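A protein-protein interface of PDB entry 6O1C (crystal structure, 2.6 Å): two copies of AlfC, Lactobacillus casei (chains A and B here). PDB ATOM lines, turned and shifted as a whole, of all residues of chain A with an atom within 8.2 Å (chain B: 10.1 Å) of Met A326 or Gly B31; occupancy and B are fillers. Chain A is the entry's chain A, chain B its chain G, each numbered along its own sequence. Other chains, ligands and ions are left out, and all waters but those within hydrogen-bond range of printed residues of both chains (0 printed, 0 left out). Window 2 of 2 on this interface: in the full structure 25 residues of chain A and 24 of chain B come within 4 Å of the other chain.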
ATOM      1  N   LEU A  72     -13.122  22.483  22.959  1.00  0.00           N
ATOM      2  CA  LEU A  72     -14.079  22.710  21.845  1.00  0.00           C
ATOM      3  C   LEU A  72     -15.139  21.617  21.886  1.00  0.00           C
ATOM      4  O   LEU A  72     -16.356  21.947  21.862  1.00  0.00           O
ATOM      5  CB  LEU A  72     -13.343  22.690  20.501  1.00  0.00           C
ATOM      6  CG  LEU A  72     -14.230  22.770  19.256  1.00  0.00           C
ATOM      7  CD1 LEU A  72     -15.149  23.996  19.298  1.00  0.00           C
ATOM      8  CD2 LEU A  72     -13.391  22.790  17.997  1.00  0.00           C
ATOM      9  N   PHE A 285      -7.958  16.167   6.431  1.00  0.00           N
ATOM     10  CA  PHE A 285      -7.938  17.583   5.983  1.00  0.00           C
ATOM     11  C   PHE A 285      -7.641  17.653   4.482  1.00  0.00           C
ATOM     12  O   PHE A 285      -6.810  16.904   3.991  1.00  0.00           O
ATOM     13  CB  PHE A 285      -6.936  18.381   6.814  1.00  0.00           C
ATOM     14  CG  PHE A 285      -6.737  19.806   6.366  1.00  0.00           C
ATOM     15  CD1 PHE A 285      -7.636  20.793   6.727  1.00  0.00           C
ATOM     16  CD2 PHE A 285      -5.656  20.151   5.567  1.00  0.00           C
ATOM     17  CE1 PHE A 285      -7.466  22.096   6.298  1.00  0.00           C
ATOM     18  CE2 PHE A 285      -5.476  21.456   5.145  1.00  0.00           C
ATOM     19  CZ  PHE A 285      -6.387  22.426   5.505  1.00  0.00           C
ATOM     20  N   GLN A 290     -14.063  22.813   0.664  1.00  0.00           N
ATOM     21  CA  GLN A 290     -14.747  23.856   1.481  1.00  0.00           C
ATOM     22  C   GLN A 290     -16.257  23.582   1.531  1.00  0.00           C
ATOM     23  O   GLN A 290     -17.003  24.516   1.840  1.00  0.00           O
ATOM     24  CB  GLN A 290     -14.491  25.246   0.892  1.00  0.00           C
ATOM     25  CG  GLN A 290     -13.024  25.618   0.782  1.00  0.00           C
ATOM     26  CD  GLN A 290     -12.324  25.631   2.120  1.00  0.00           C
ATOM     27  OE1 GLN A 290     -12.906  25.992   3.138  1.00  0.00           O
ATOM     28  NE2 GLN A 290     -11.055  25.239   2.131  1.00  0.00           N
ATOM     29  N   TRP A 292     -18.410  22.530   3.636  1.00  0.00           N
ATOM     30  CA  TRP A 292     -18.803  22.385   5.059  1.00  0.00           C
ATOM     31  C   TRP A 292     -20.327  22.324   5.179  1.00  0.00           C
ATOM     32  O   TRP A 292     -20.990  23.266   4.722  1.00  0.00           O
ATOM     33  CB  TRP A 292     -18.265  23.557   5.872  1.00  0.00           C
ATOM     34  CG  TRP A 292     -16.797  23.772   5.720  1.00  0.00           C
ATOM     35  CD1 TRP A 292     -16.190  24.754   4.999  1.00  0.00           C
ATOM     36  CD2 TRP A 292     -15.748  22.979   6.294  1.00  0.00           C
ATOM     37  NE1 TRP A 292     -14.830  24.622   5.085  1.00  0.00           N
ATOM     38  CE2 TRP A 292     -14.528  23.539   5.870  1.00  0.00           C
ATOM     39  CE3 TRP A 292     -15.715  21.842   7.107  1.00  0.00           C
ATOM     40  CZ2 TRP A 292     -13.291  23.008   6.246  1.00  0.00           C
ATOM     41  CZ3 TRP A 292     -14.490  21.309   7.472  1.00  0.00           C
ATOM     42  CH2 TRP A 292     -13.300  21.891   7.051  1.00  0.00           C
ATOM     43  N   ASP A 319      -5.453  20.140  10.581  1.00  0.00           N
ATOM     44  CA  ASP A 319      -4.613  20.701   9.480  1.00  0.00           C
ATOM     45  C   ASP A 319      -3.138  20.423   9.791  1.00  0.00           C
ATOM     46  O   ASP A 319      -2.796  19.871  10.840  1.00  0.00           O
ATOM     47  CB  ASP A 319      -4.947  22.169   9.230  1.00  0.00           C
ATOM     48  CG  ASP A 319      -4.273  23.165  10.169  1.00  0.00           C
ATOM     49  OD1 ASP A 319      -3.603  22.725  11.138  1.00  0.00           O
ATOM     50  OD2 ASP A 319      -4.463  24.397   9.933  1.00  0.00           O
ATOM     51  N   ARG A 323      -4.377  22.210  13.794  1.00  0.00           N
ATOM     52  CA  ARG A 323      -5.542  23.085  14.084  1.00  0.00           C
ATOM     53  C   ARG A 323      -6.829  22.431  13.565  1.00  0.00           C
ATOM     54  O   ARG A 323      -6.808  21.782  12.480  1.00  0.00           O
ATOM     55  CB  ARG A 323      -5.346  24.454  13.449  1.00  0.00           C
ATOM     56  CG  ARG A 323      -4.107  25.162  13.982  1.00  0.00           C
ATOM     57  CD  ARG A 323      -3.850  26.525  13.372  1.00  0.00           C
ATOM     58  NE  ARG A 323      -3.773  26.432  11.924  1.00  0.00           N
ATOM     59  CZ  ARG A 323      -3.468  27.435  11.124  1.00  0.00           C
ATOM     60  NH1 ARG A 323      -3.081  28.602  11.619  1.00  0.00           N
ATOM     61  NH2 ARG A 323      -3.482  27.249   9.822  1.00  0.00           N
ATOM     62  N   VAL A 324      -7.895  22.574  14.344  1.00  0.00           N
ATOM     63  CA  VAL A 324      -9.287  22.464  13.852  1.00  0.00           C
ATOM     64  C   VAL A 324      -9.477  23.570  12.823  1.00  0.00           C
ATOM     65  O   VAL A 324      -9.316  24.727  13.158  1.00  0.00           O
ATOM     66  CB  VAL A 324     -10.293  22.589  15.009  1.00  0.00           C
ATOM     67  CG1 VAL A 324     -11.725  22.570  14.488  1.00  0.00           C
ATOM     68  CG2 VAL A 324     -10.092  21.500  16.053  1.00  0.00           C
ATOM     69  N   PRO A 325      -9.792  23.266  11.546  1.00  0.00           N
ATOM     70  CA  PRO A 325     -10.110  24.290  10.555  1.00  0.00           C
ATOM     71  C   PRO A 325     -11.130  25.320  11.061  1.00  0.00           C
ATOM     72  O   PRO A 325     -12.088  24.955  11.711  1.00  0.00           O
ATOM     73  CB  PRO A 325     -10.713  23.455   9.409  1.00  0.00           C
ATOM     74  CG  PRO A 325      -9.939  22.174   9.470  1.00  0.00           C
ATOM     75  CD  PRO A 325      -9.849  21.910  10.964  1.00  0.00           C
ATOM     76  N   MET A 326     -10.876  26.590  10.748  1.00  0.00           N
ATOM     77  CA  MET A 326     -11.700  27.743  11.203  1.00  0.00           C
ATOM     78  C   MET A 326     -13.183  27.465  10.920  1.00  0.00           C
ATOM     79  O   MET A 326     -14.010  27.632  11.834  1.00  0.00           O
ATOM     80  CB  MET A 326     -11.238  29.017  10.502  1.00  0.00           C
ATOM     81  CG  MET A 326     -12.227  30.138  10.550  1.00  0.00           C
ATOM     82  SD  MET A 326     -11.745  31.669   9.633  1.00  0.00           S
ATOM     83  CE  MET A 326     -10.660  31.008   8.355  1.00  0.00           C
ATOM     84  N   MET A 327     -13.506  27.007   9.718  1.00  0.00           N
ATOM     85  CA  MET A 327     -14.931  26.820   9.319  1.00  0.00           C
ATOM     86  C   MET A 327     -15.558  25.618  10.040  1.00  0.00           C
ATOM     87  O   MET A 327     -16.756  25.693  10.386  1.00  0.00           O
ATOM     88  CB  MET A 327     -15.080  26.691   7.804  1.00  0.00           C
ATOM     89  CG  MET A 327     -15.109  28.035   7.103  1.00  0.00           C
ATOM     90  SD  MET A 327     -16.187  29.232   7.965  1.00  0.00           S
ATOM     91  CE  MET A 327     -17.833  28.529   7.735  1.00  0.00           C
ATOM     92  N   ALA A 328     -14.799  24.567  10.318  1.00  0.00           N
ATOM     93  CA  ALA A 328     -15.273  23.433  11.145  1.00  0.00           C
ATOM     94  C   ALA A 328     -15.594  23.930  12.554  1.00  0.00           C
ATOM     95  O   ALA A 328     -16.644  23.581  13.093  1.00  0.00           O
ATOM     96  CB  ALA A 328     -14.270  22.311  11.177  1.00  0.00           C
ATOM     97  N   GLU A 329     -14.715  24.733  13.145  1.00  0.00           N
ATOM     98  CA  GLU A 329     -14.911  25.245  14.525  1.00  0.00           C
ATOM     99  C   GLU A 329     -16.166  26.127  14.552  1.00  0.00           C
ATOM    100  O   GLU A 329     -17.002  25.926  15.464  1.00  0.00           O
ATOM    101  CB  GLU A 329     -13.662  25.974  15.021  1.00  0.00           C
ATOM    102  CG  GLU A 329     -13.832  26.490  16.442  1.00  0.00           C
ATOM    103  CD  GLU A 329     -12.656  27.282  16.999  1.00  0.00           C
ATOM    104  OE1 GLU A 329     -11.498  26.845  16.717  1.00  0.00           O
ATOM    105  OE2 GLU A 329     -12.884  28.337  17.701  1.00  0.00           O
ATOM    106  N   GLU A 330     -16.289  27.059  13.601  1.00  0.00           N
ATOM    107  CA  GLU A 330     -17.474  27.965  13.472  1.00  0.00           C
ATOM    108  C   GLU A 330     -18.770  27.146  13.377  1.00  0.00           C
ATOM    109  O   GLU A 330     -19.731  27.459  14.109  1.00  0.00           O
ATOM    110  CB  GLU A 330     -17.365  28.863  12.237  1.00  0.00           C
ATOM    111  CG  GLU A 330     -16.543  30.112  12.464  1.00  0.00           C
ATOM    112  CD  GLU A 330     -16.726  31.192  11.414  1.00  0.00           C
ATOM    113  OE1 GLU A 330     -17.890  31.466  10.988  1.00  0.00           O
ATOM    114  OE2 GLU A 330     -15.697  31.789  11.045  1.00  0.00           O
ATOM    115  N   ASN A 331     -18.790  26.130  12.515  1.00  0.00           N
ATOM    116  CA  ASN A 331     -20.027  25.369  12.232  1.00  0.00           C
ATOM    117  C   ASN A 331     -20.410  24.524  13.461  1.00  0.00           C
ATOM    118  O   ASN A 331     -21.632  24.430  13.749  1.00  0.00           O
ATOM    119  CB  ASN A 331     -19.905  24.568  10.940  1.00  0.00           C
ATOM    120  CG  ASN A 331     -19.966  25.461   9.717  1.00  0.00           C
ATOM    121  OD1 ASN A 331     -19.747  26.662   9.805  1.00  0.00           O
ATOM    122  ND2 ASN A 331     -20.253  24.898   8.563  1.00  0.00           N
ATOM    123  N   LEU A 332     -19.435  23.970  14.186  1.00  0.00           N
ATOM    124  CA  LEU A 332     -19.700  23.179  15.413  1.00  0.00           C
ATOM    125  C   LEU A 332     -20.333  24.087  16.471  1.00  0.00           C
ATOM    126  O   LEU A 332     -21.332  23.697  17.083  1.00  0.00           O
ATOM    127  CB  LEU A 332     -18.391  22.557  15.921  1.00  0.00           C
ATOM    128  CG  LEU A 332     -17.871  21.345  15.152  1.00  0.00           C
ATOM    129  CD1 LEU A 332     -16.480  20.970  15.626  1.00  0.00           C
ATOM    130  CD2 LEU A 332     -18.826  20.171  15.258  1.00  0.00           C
ATOM    131  N   LEU A 333     -19.772  25.268  16.666  1.00  0.00           N
ATOM    132  CA  LEU A 333     -20.223  26.223  17.721  1.00  0.00           C
ATOM    133  C   LEU A 333     -21.609  26.760  17.378  1.00  0.00           C
ATOM    134  O   LEU A 333     -22.431  26.845  18.286  1.00  0.00           O
ATOM    135  CB  LEU A 333     -19.181  27.335  17.895  1.00  0.00           C
ATOM    136  CG  LEU A 333     -17.900  26.857  18.584  1.00  0.00           C
ATOM    137  CD1 LEU A 333     -16.802  27.889  18.467  1.00  0.00           C
ATOM    138  CD2 LEU A 333     -18.143  26.510  20.046  1.00  0.00           C
ATOM    139  N   LEU B  25       0.844  29.612   8.000  1.00  0.00           N
ATOM    140  CA  LEU B  25      -0.420  29.936   8.721  1.00  0.00           C
ATOM    141  C   LEU B  25      -1.599  29.907   7.739  1.00  0.00           C
ATOM    142  O   LEU B  25      -2.743  29.704   8.193  1.00  0.00           O
ATOM    143  CB  LEU B  25      -0.297  31.296   9.407  1.00  0.00           C
ATOM    144  CG  LEU B  25       0.495  31.297  10.715  1.00  0.00           C
ATOM    145  CD1 LEU B  25       0.732  32.727  11.209  1.00  0.00           C
ATOM    146  CD2 LEU B  25      -0.204  30.468  11.781  1.00  0.00           C
ATOM    147  N   ALA B  26      -1.341  30.160   6.454  1.00  0.00           N
ATOM    148  CA  ALA B  26      -2.300  29.986   5.342  1.00  0.00           C
ATOM    149  C   ALA B  26      -3.645  30.702   5.599  1.00  0.00           C
ATOM    150  O   ALA B  26      -4.694  30.114   5.310  1.00  0.00           O
ATOM    151  CB  ALA B  26      -2.473  28.506   5.115  1.00  0.00           C
ATOM    152  N   GLY B  27      -3.626  31.950   6.063  1.00  0.00           N
ATOM    153  CA  GLY B  27      -4.807  32.842   6.110  1.00  0.00           C
ATOM    154  C   GLY B  27      -5.635  32.656   7.370  1.00  0.00           C
ATOM    155  O   GLY B  27      -6.736  33.257   7.462  1.00  0.00           O
ATOM    156  N   GLU B  28      -5.106  31.894   8.331  1.00  0.00           N
ATOM    157  CA  GLU B  28      -5.840  31.456   9.543  1.00  0.00           C
ATOM    158  C   GLU B  28      -4.936  31.610  10.762  1.00  0.00           C
ATOM    159  O   GLU B  28      -3.753  31.254  10.654  1.00  0.00           O
ATOM    160  CB  GLU B  28      -6.221  29.990   9.324  1.00  0.00           C
ATOM    161  CG  GLU B  28      -7.507  29.547   9.975  1.00  0.00           C
ATOM    162  CD  GLU B  28      -8.130  28.391   9.203  1.00  0.00           C
ATOM    163  OE1 GLU B  28      -8.661  28.681   8.081  1.00  0.00           O
ATOM    164  OE2 GLU B  28      -8.063  27.219   9.688  1.00  0.00           O
ATOM    165  N   TYR B  29      -5.461  32.123  11.875  1.00  0.00           N
ATOM    166  CA  TYR B  29      -4.726  32.201  13.158  1.00  0.00           C
ATOM    167  C   TYR B  29      -5.719  32.090  14.308  1.00  0.00           C
ATOM    168  O   TYR B  29      -6.602  32.959  14.431  1.00  0.00           O
ATOM    169  CB  TYR B  29      -3.911  33.498  13.271  1.00  0.00           C
ATOM    170  CG  TYR B  29      -3.097  33.573  14.530  1.00  0.00           C
ATOM    171  CD1 TYR B  29      -1.900  32.872  14.647  1.00  0.00           C
ATOM    172  CD2 TYR B  29      -3.525  34.316  15.619  1.00  0.00           C
ATOM    173  CE1 TYR B  29      -1.150  32.915  15.812  1.00  0.00           C
ATOM    174  CE2 TYR B  29      -2.780  34.368  16.791  1.00  0.00           C
ATOM    175  CZ  TYR B  29      -1.588  33.672  16.884  1.00  0.00           C
ATOM    176  OH  TYR B  29      -0.852  33.736  18.026  1.00  0.00           O
ATOM    177  N   ARG B  30      -5.557  31.044  15.115  1.00  0.00           N
ATOM    178  CA  ARG B  30      -6.357  30.724  16.322  1.00  0.00           C
ATOM    179  C   ARG B  30      -7.850  30.896  16.045  1.00  0.00           C
ATOM    180  O   ARG B  30      -8.501  31.649  16.804  1.00  0.00           O
ATOM    181  CB  ARG B  30      -5.926  31.607  17.487  1.00  0.00           C
ATOM    182  CG  ARG B  30      -4.497  31.353  17.921  1.00  0.00           C
ATOM    183  CD  ARG B  30      -4.195  32.099  19.210  1.00  0.00           C
ATOM    184  NE  ARG B  30      -2.781  32.063  19.528  1.00  0.00           N
ATOM    185  CZ  ARG B  30      -2.134  31.010  20.030  1.00  0.00           C
ATOM    186  NH1 ARG B  30      -2.741  29.867  20.257  1.00  0.00           N
ATOM    187  NH2 ARG B  30      -0.851  31.105  20.298  1.00  0.00           N
ATOM    188  N   GLY B  31      -8.356  30.236  14.999  1.00  0.00           N
ATOM    189  CA  GLY B  31      -9.795  30.144  14.716  1.00  0.00           C
ATOM    190  C   GLY B  31     -10.347  31.357  13.999  1.00  0.00           C
ATOM    191  O   GLY B  31     -11.574  31.415  13.816  1.00  0.00           O
ATOM    192  N   GLU B  32      -9.483  32.265  13.557  1.00  0.00           N
ATOM    193  CA  GLU B  32      -9.899  33.523  12.902  1.00  0.00           C
ATOM    194  C   GLU B  32      -9.149  33.747  11.598  1.00  0.00           C
ATOM    195  O   GLU B  32      -8.025  33.246  11.410  1.00  0.00           O
ATOM    196  CB  GLU B  32      -9.738  34.670  13.886  1.00  0.00           C
ATOM    197  CG  GLU B  32     -10.883  34.680  14.850  1.00  0.00           C
ATOM    198  CD  GLU B  32     -10.654  35.480  16.104  1.00  0.00           C
ATOM    199  OE1 GLU B  32      -9.694  36.313  16.124  1.00  0.00           O
ATOM    200  OE2 GLU B  32     -11.434  35.250  17.049  1.00  0.00           O
ATOM    201  N   SER B  33      -9.806  34.505  10.736  1.00  0.00           N
ATOM    202  CA  SER B  33      -9.422  34.763   9.334  1.00  0.00           C
ATOM    203  C   SER B  33      -8.497  35.981   9.256  1.00  0.00           C
ATOM    204  O   SER B  33      -8.780  36.998   9.918  1.00  0.00           O
ATOM    205  CB  SER B  33     -10.656  34.976   8.511  1.00  0.00           C
ATOM    206  OG  SER B  33     -10.321  35.119   7.145  1.00  0.00           O
ATOM    207  N   SER B  34      -7.455  35.891   8.435  1.00  0.00           N
ATOM    208  CA  SER B  34      -6.693  37.075   7.979  1.00  0.00           C
ATOM    209  C   SER B  34      -7.640  37.974   7.197  1.00  0.00           C
ATOM    210  O   SER B  34      -8.756  37.523   6.914  1.00  0.00           O
ATOM    211  CB  SER B  34      -5.536  36.682   7.130  1.00  0.00           C
ATOM    212  OG  SER B  34      -5.996  36.142   5.908  1.00  0.00           O
ATOM    213  N   SER B  35      -7.194  39.173   6.822  1.00  0.00           N
ATOM    214  CA  SER B  35      -7.822  39.977   5.739  1.00  0.00           C
ATOM    215  C   SER B  35      -7.611  39.244   4.405  1.00  0.00           C
ATOM    216  O   SER B  35      -6.977  38.174   4.408  1.00  0.00           O
ATOM    217  CB  SER B  35      -7.240  41.360   5.693  1.00  0.00           C
ATOM    218  OG  SER B  35      -5.951  41.332   5.090  1.00  0.00           O
ATOM    219  N   ALA B  38      -3.335  37.496   3.170  1.00  0.00           N
ATOM    220  CA  ALA B  38      -2.876  36.474   4.140  1.00  0.00           C
ATOM    221  C   ALA B  38      -1.421  36.756   4.549  1.00  0.00           C
ATOM    222  O   ALA B  38      -1.082  36.450   5.702  1.00  0.00           O
ATOM    223  CB  ALA B  38      -3.046  35.101   3.533  1.00  0.00           C
ATOM    224  N   ILE B  41      -0.624  38.628   7.811  1.00  0.00           N
ATOM    225  CA  ILE B  41      -1.303  37.983   8.976  1.00  0.00           C
ATOM    226  C   ILE B  41      -0.610  38.388  10.284  1.00  0.00           C
ATOM    227  O   ILE B  41      -1.334  38.505  11.311  1.00  0.00           O
ATOM    228  CB  ILE B  41      -1.393  36.460   8.818  1.00  0.00           C
ATOM    229  CG1 ILE B  41      -2.371  35.857   9.828  1.00  0.00           C
ATOM    230  CG2 ILE B  41      -0.019  35.810   8.900  1.00  0.00           C
ATOM    231  CD1 ILE B  41      -2.877  34.475   9.435  1.00  0.00           C
ATOM    232  N   LYS B  44      -2.000  41.658  11.265  1.00  0.00           N
ATOM    233  CA  LYS B  44      -3.453  41.441  11.466  1.00  0.00           C
ATOM    234  C   LYS B  44      -3.729  41.012  12.909  1.00  0.00           C
ATOM    235  O   LYS B  44      -4.673  41.551  13.503  1.00  0.00           O
ATOM    236  CB  LYS B  44      -3.963  40.386  10.482  1.00  0.00           C
ATOM    237  CG  LYS B  44      -5.447  40.057  10.574  1.00  0.00           C
ATOM    238  CD  LYS B  44      -6.331  41.253  10.379  1.00  0.00           C
ATOM    239  CE  LYS B  44      -7.785  40.908  10.181  1.00  0.00           C
ATOM    240  NZ  LYS B  44      -8.574  42.166  10.060  1.00  0.00           N
ATOM    241  N   PHE B  45      -2.931  40.087  13.446  1.00  0.00           N
ATOM    242  CA  PHE B  45      -3.140  39.486  14.790  1.00  0.00           C
ATOM    243  C   PHE B  45      -2.055  39.923  15.786  1.00  0.00           C
ATOM    244  O   PHE B  45      -2.106  39.468  16.951  1.00  0.00           O
ATOM    245  CB  PHE B  45      -3.258  37.967  14.653  1.00  0.00           C
ATOM    246  CG  PHE B  45      -4.518  37.552  13.936  1.00  0.00           C
ATOM    247  CD1 PHE B  45      -5.754  37.716  14.543  1.00  0.00           C
ATOM    248  CD2 PHE B  45      -4.471  37.082  12.632  1.00  0.00           C
ATOM    249  CE1 PHE B  45      -6.924  37.405  13.868  1.00  0.00           C
ATOM    250  CE2 PHE B  45      -5.644  36.744  11.969  1.00  0.00           C
ATOM    251  CZ  PHE B  45      -6.863  36.894  12.589  1.00  0.00           C
ATOM    252  N   SER B 286      -3.547  31.142   1.079  1.00  0.00           N
ATOM    253  CA  SER B 286      -4.694  31.191   2.028  1.00  0.00           C
ATOM    254  C   SER B 286      -5.625  30.019   1.729  1.00  0.00           C
ATOM    255  O   SER B 286      -6.189  30.011   0.657  1.00  0.00           O
ATOM    256  CB  SER B 286      -5.427  32.522   1.877  1.00  0.00           C
ATOM    257  OG  SER B 286      -6.507  32.625   2.779  1.00  0.00           O
ATOM    258  N   TYR B 287      -5.752  29.054   2.638  1.00  0.00           N
ATOM    259  CA  TYR B 287      -6.643  27.870   2.507  1.00  0.00           C
ATOM    260  C   TYR B 287      -8.076  28.361   2.259  1.00  0.00           C
ATOM    261  O   TYR B 287      -8.753  27.869   1.353  1.00  0.00           O
ATOM    262  CB  TYR B 287      -6.710  27.025   3.795  1.00  0.00           C
ATOM    263  CG  TYR B 287      -5.497  26.234   4.243  1.00  0.00           C
ATOM    264  CD1 TYR B 287      -4.718  25.525   3.346  1.00  0.00           C
ATOM    265  CD2 TYR B 287      -5.166  26.128   5.590  1.00  0.00           C
ATOM    266  CE1 TYR B 287      -3.621  24.790   3.762  1.00  0.00           C
ATOM    267  CE2 TYR B 287      -4.081  25.381   6.027  1.00  0.00           C
ATOM    268  CZ  TYR B 287      -3.289  24.729   5.102  1.00  0.00           C
ATOM    269  OH  TYR B 287      -2.185  24.009   5.464  1.00  0.00           O
ATOM    270  N   HIS B 288      -8.520  29.339   3.049  1.00  0.00           N
ATOM    271  CA  HIS B 288      -9.940  29.799   3.041  1.00  0.00           C
ATOM    272  C   HIS B 288     -10.269  30.534   1.731  1.00  0.00           C
ATOM    273  O   HIS B 288     -11.430  30.516   1.373  1.00  0.00           O
ATOM    274  CB  HIS B 288     -10.327  30.562   4.324  1.00  0.00           C
ATOM    275  CG  HIS B 288      -9.857  31.969   4.434  1.00  0.00           C
ATOM    276  ND1 HIS B 288     -10.528  33.073   3.902  1.00  0.00           N
ATOM    277  CD2 HIS B 288      -8.748  32.458   5.028  1.00  0.00           C
ATOM    278  CE1 HIS B 288      -9.875  34.177   4.205  1.00  0.00           C
ATOM    279  NE2 HIS B 288      -8.771  33.835   4.898  1.00  0.00           N
ATOM    280  N   ASP B 289      -9.291  31.087   0.996  1.00  0.00           N
ATOM    281  CA  ASP B 289      -9.551  31.852  -0.253  1.00  0.00           C
ATOM    282  C   ASP B 289      -9.543  30.925  -1.476  1.00  0.00           C
ATOM    283  O   ASP B 289      -8.482  30.740  -2.071  1.00  0.00           O
ATOM    284  CB  ASP B 289      -8.540  32.988  -0.412  1.00  0.00           C
ATOM    285  CG  ASP B 289      -8.804  33.921  -1.585  1.00  0.00           C
ATOM    286  OD1 ASP B 289      -9.730  33.631  -2.365  1.00  0.00           O
ATOM    287  OD2 ASP B 289      -8.074  34.938  -1.696  1.00  0.00           O
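The backbone carbonyl oxygen (O) of Leu B25 lies within hydrogen-bond range of the guanidinium group (NH2) of Arg A323 (3.0 Å).
The backbone carbonyl oxygen of Glu B28 sits at hydrogen-bond distance from the guanidinium group of Arg A323, 2.9 Å away.
The backbone NH of Met A326 is in hydrogen-bond range of the side-chain carboxylate of Glu B28, 3.1 Å away.
The backbone NH of Ser B33 is in hydrogen-bond range of the side-chain sulfur of Met A326 (3.6 Å).
The indole nitrogen (NE1) of Trp A292 lies within hydrogen-bond range of the side-chain amide oxygen (OE1) of Gln A290 (3.1 Å).
The guanidinium group of Arg A323 is in salt-bridge range of the side-chain carboxylate of Asp A319 (2.9 Å).
O of Ala B26 lies within hydrogen-bond range of N of Tyr B287, 3.1 Å away.
NE2 of His B288 sits at hydrogen-bond distance from OG of Ser B33 (3.0 Å).
CZ of Phe A285 touches CE2 of Tyr B287, at 3.8 Å.
NE2 of Gln A290 touches O of Tyr B287, 3.6 Å away.
CA of Pro A325 touches OE2 of Glu B28, 3.7 Å away.
Met A326 touches Gly B31.
Met A326 touches Glu B32 (SD to C, 3.9 Å).
Printed residues of chain B within 4 Å of Met A326: Glu B28 (3.1 Å), Gly B31 (3.6 Å), Glu B32 (3.9 Å) and Ser B33 (3.6 Å).
No residue of chain B comes within 4 Å of Ala A328.
No residue of chain B comes within 4 Å of Glu A329.
Of the printed residues of chain B, Gln A290 touches Tyr B287 (3.6 Å).
Printed residues of chain B within 4 Å of Phe A285: Tyr B287 (3.8 Å).
Of the printed residues of chain A, Glu B32 touches Met A326.
Of the printed residues of chain B, Pro A325 touches Glu B28 (3.7 Å).
Of the printed residues of chain A, Tyr B287 touches Phe A285 and Gln A290.
The nearest residue of chain A that does not touch Gly B31 is Glu A329 (4.2 Å).
The nearest printed residue of chain A that does not touch Ser B33 is Glu A330 (6.5 Å).
Of the 19 printed residues of chain B, 6 touch a printed residue of chain A.
Hydrophobic or aromatic side chains of chain B within 4 Å of the printed part of chain A: Leu B25 and Tyr B287.
No position is printed for both chains.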
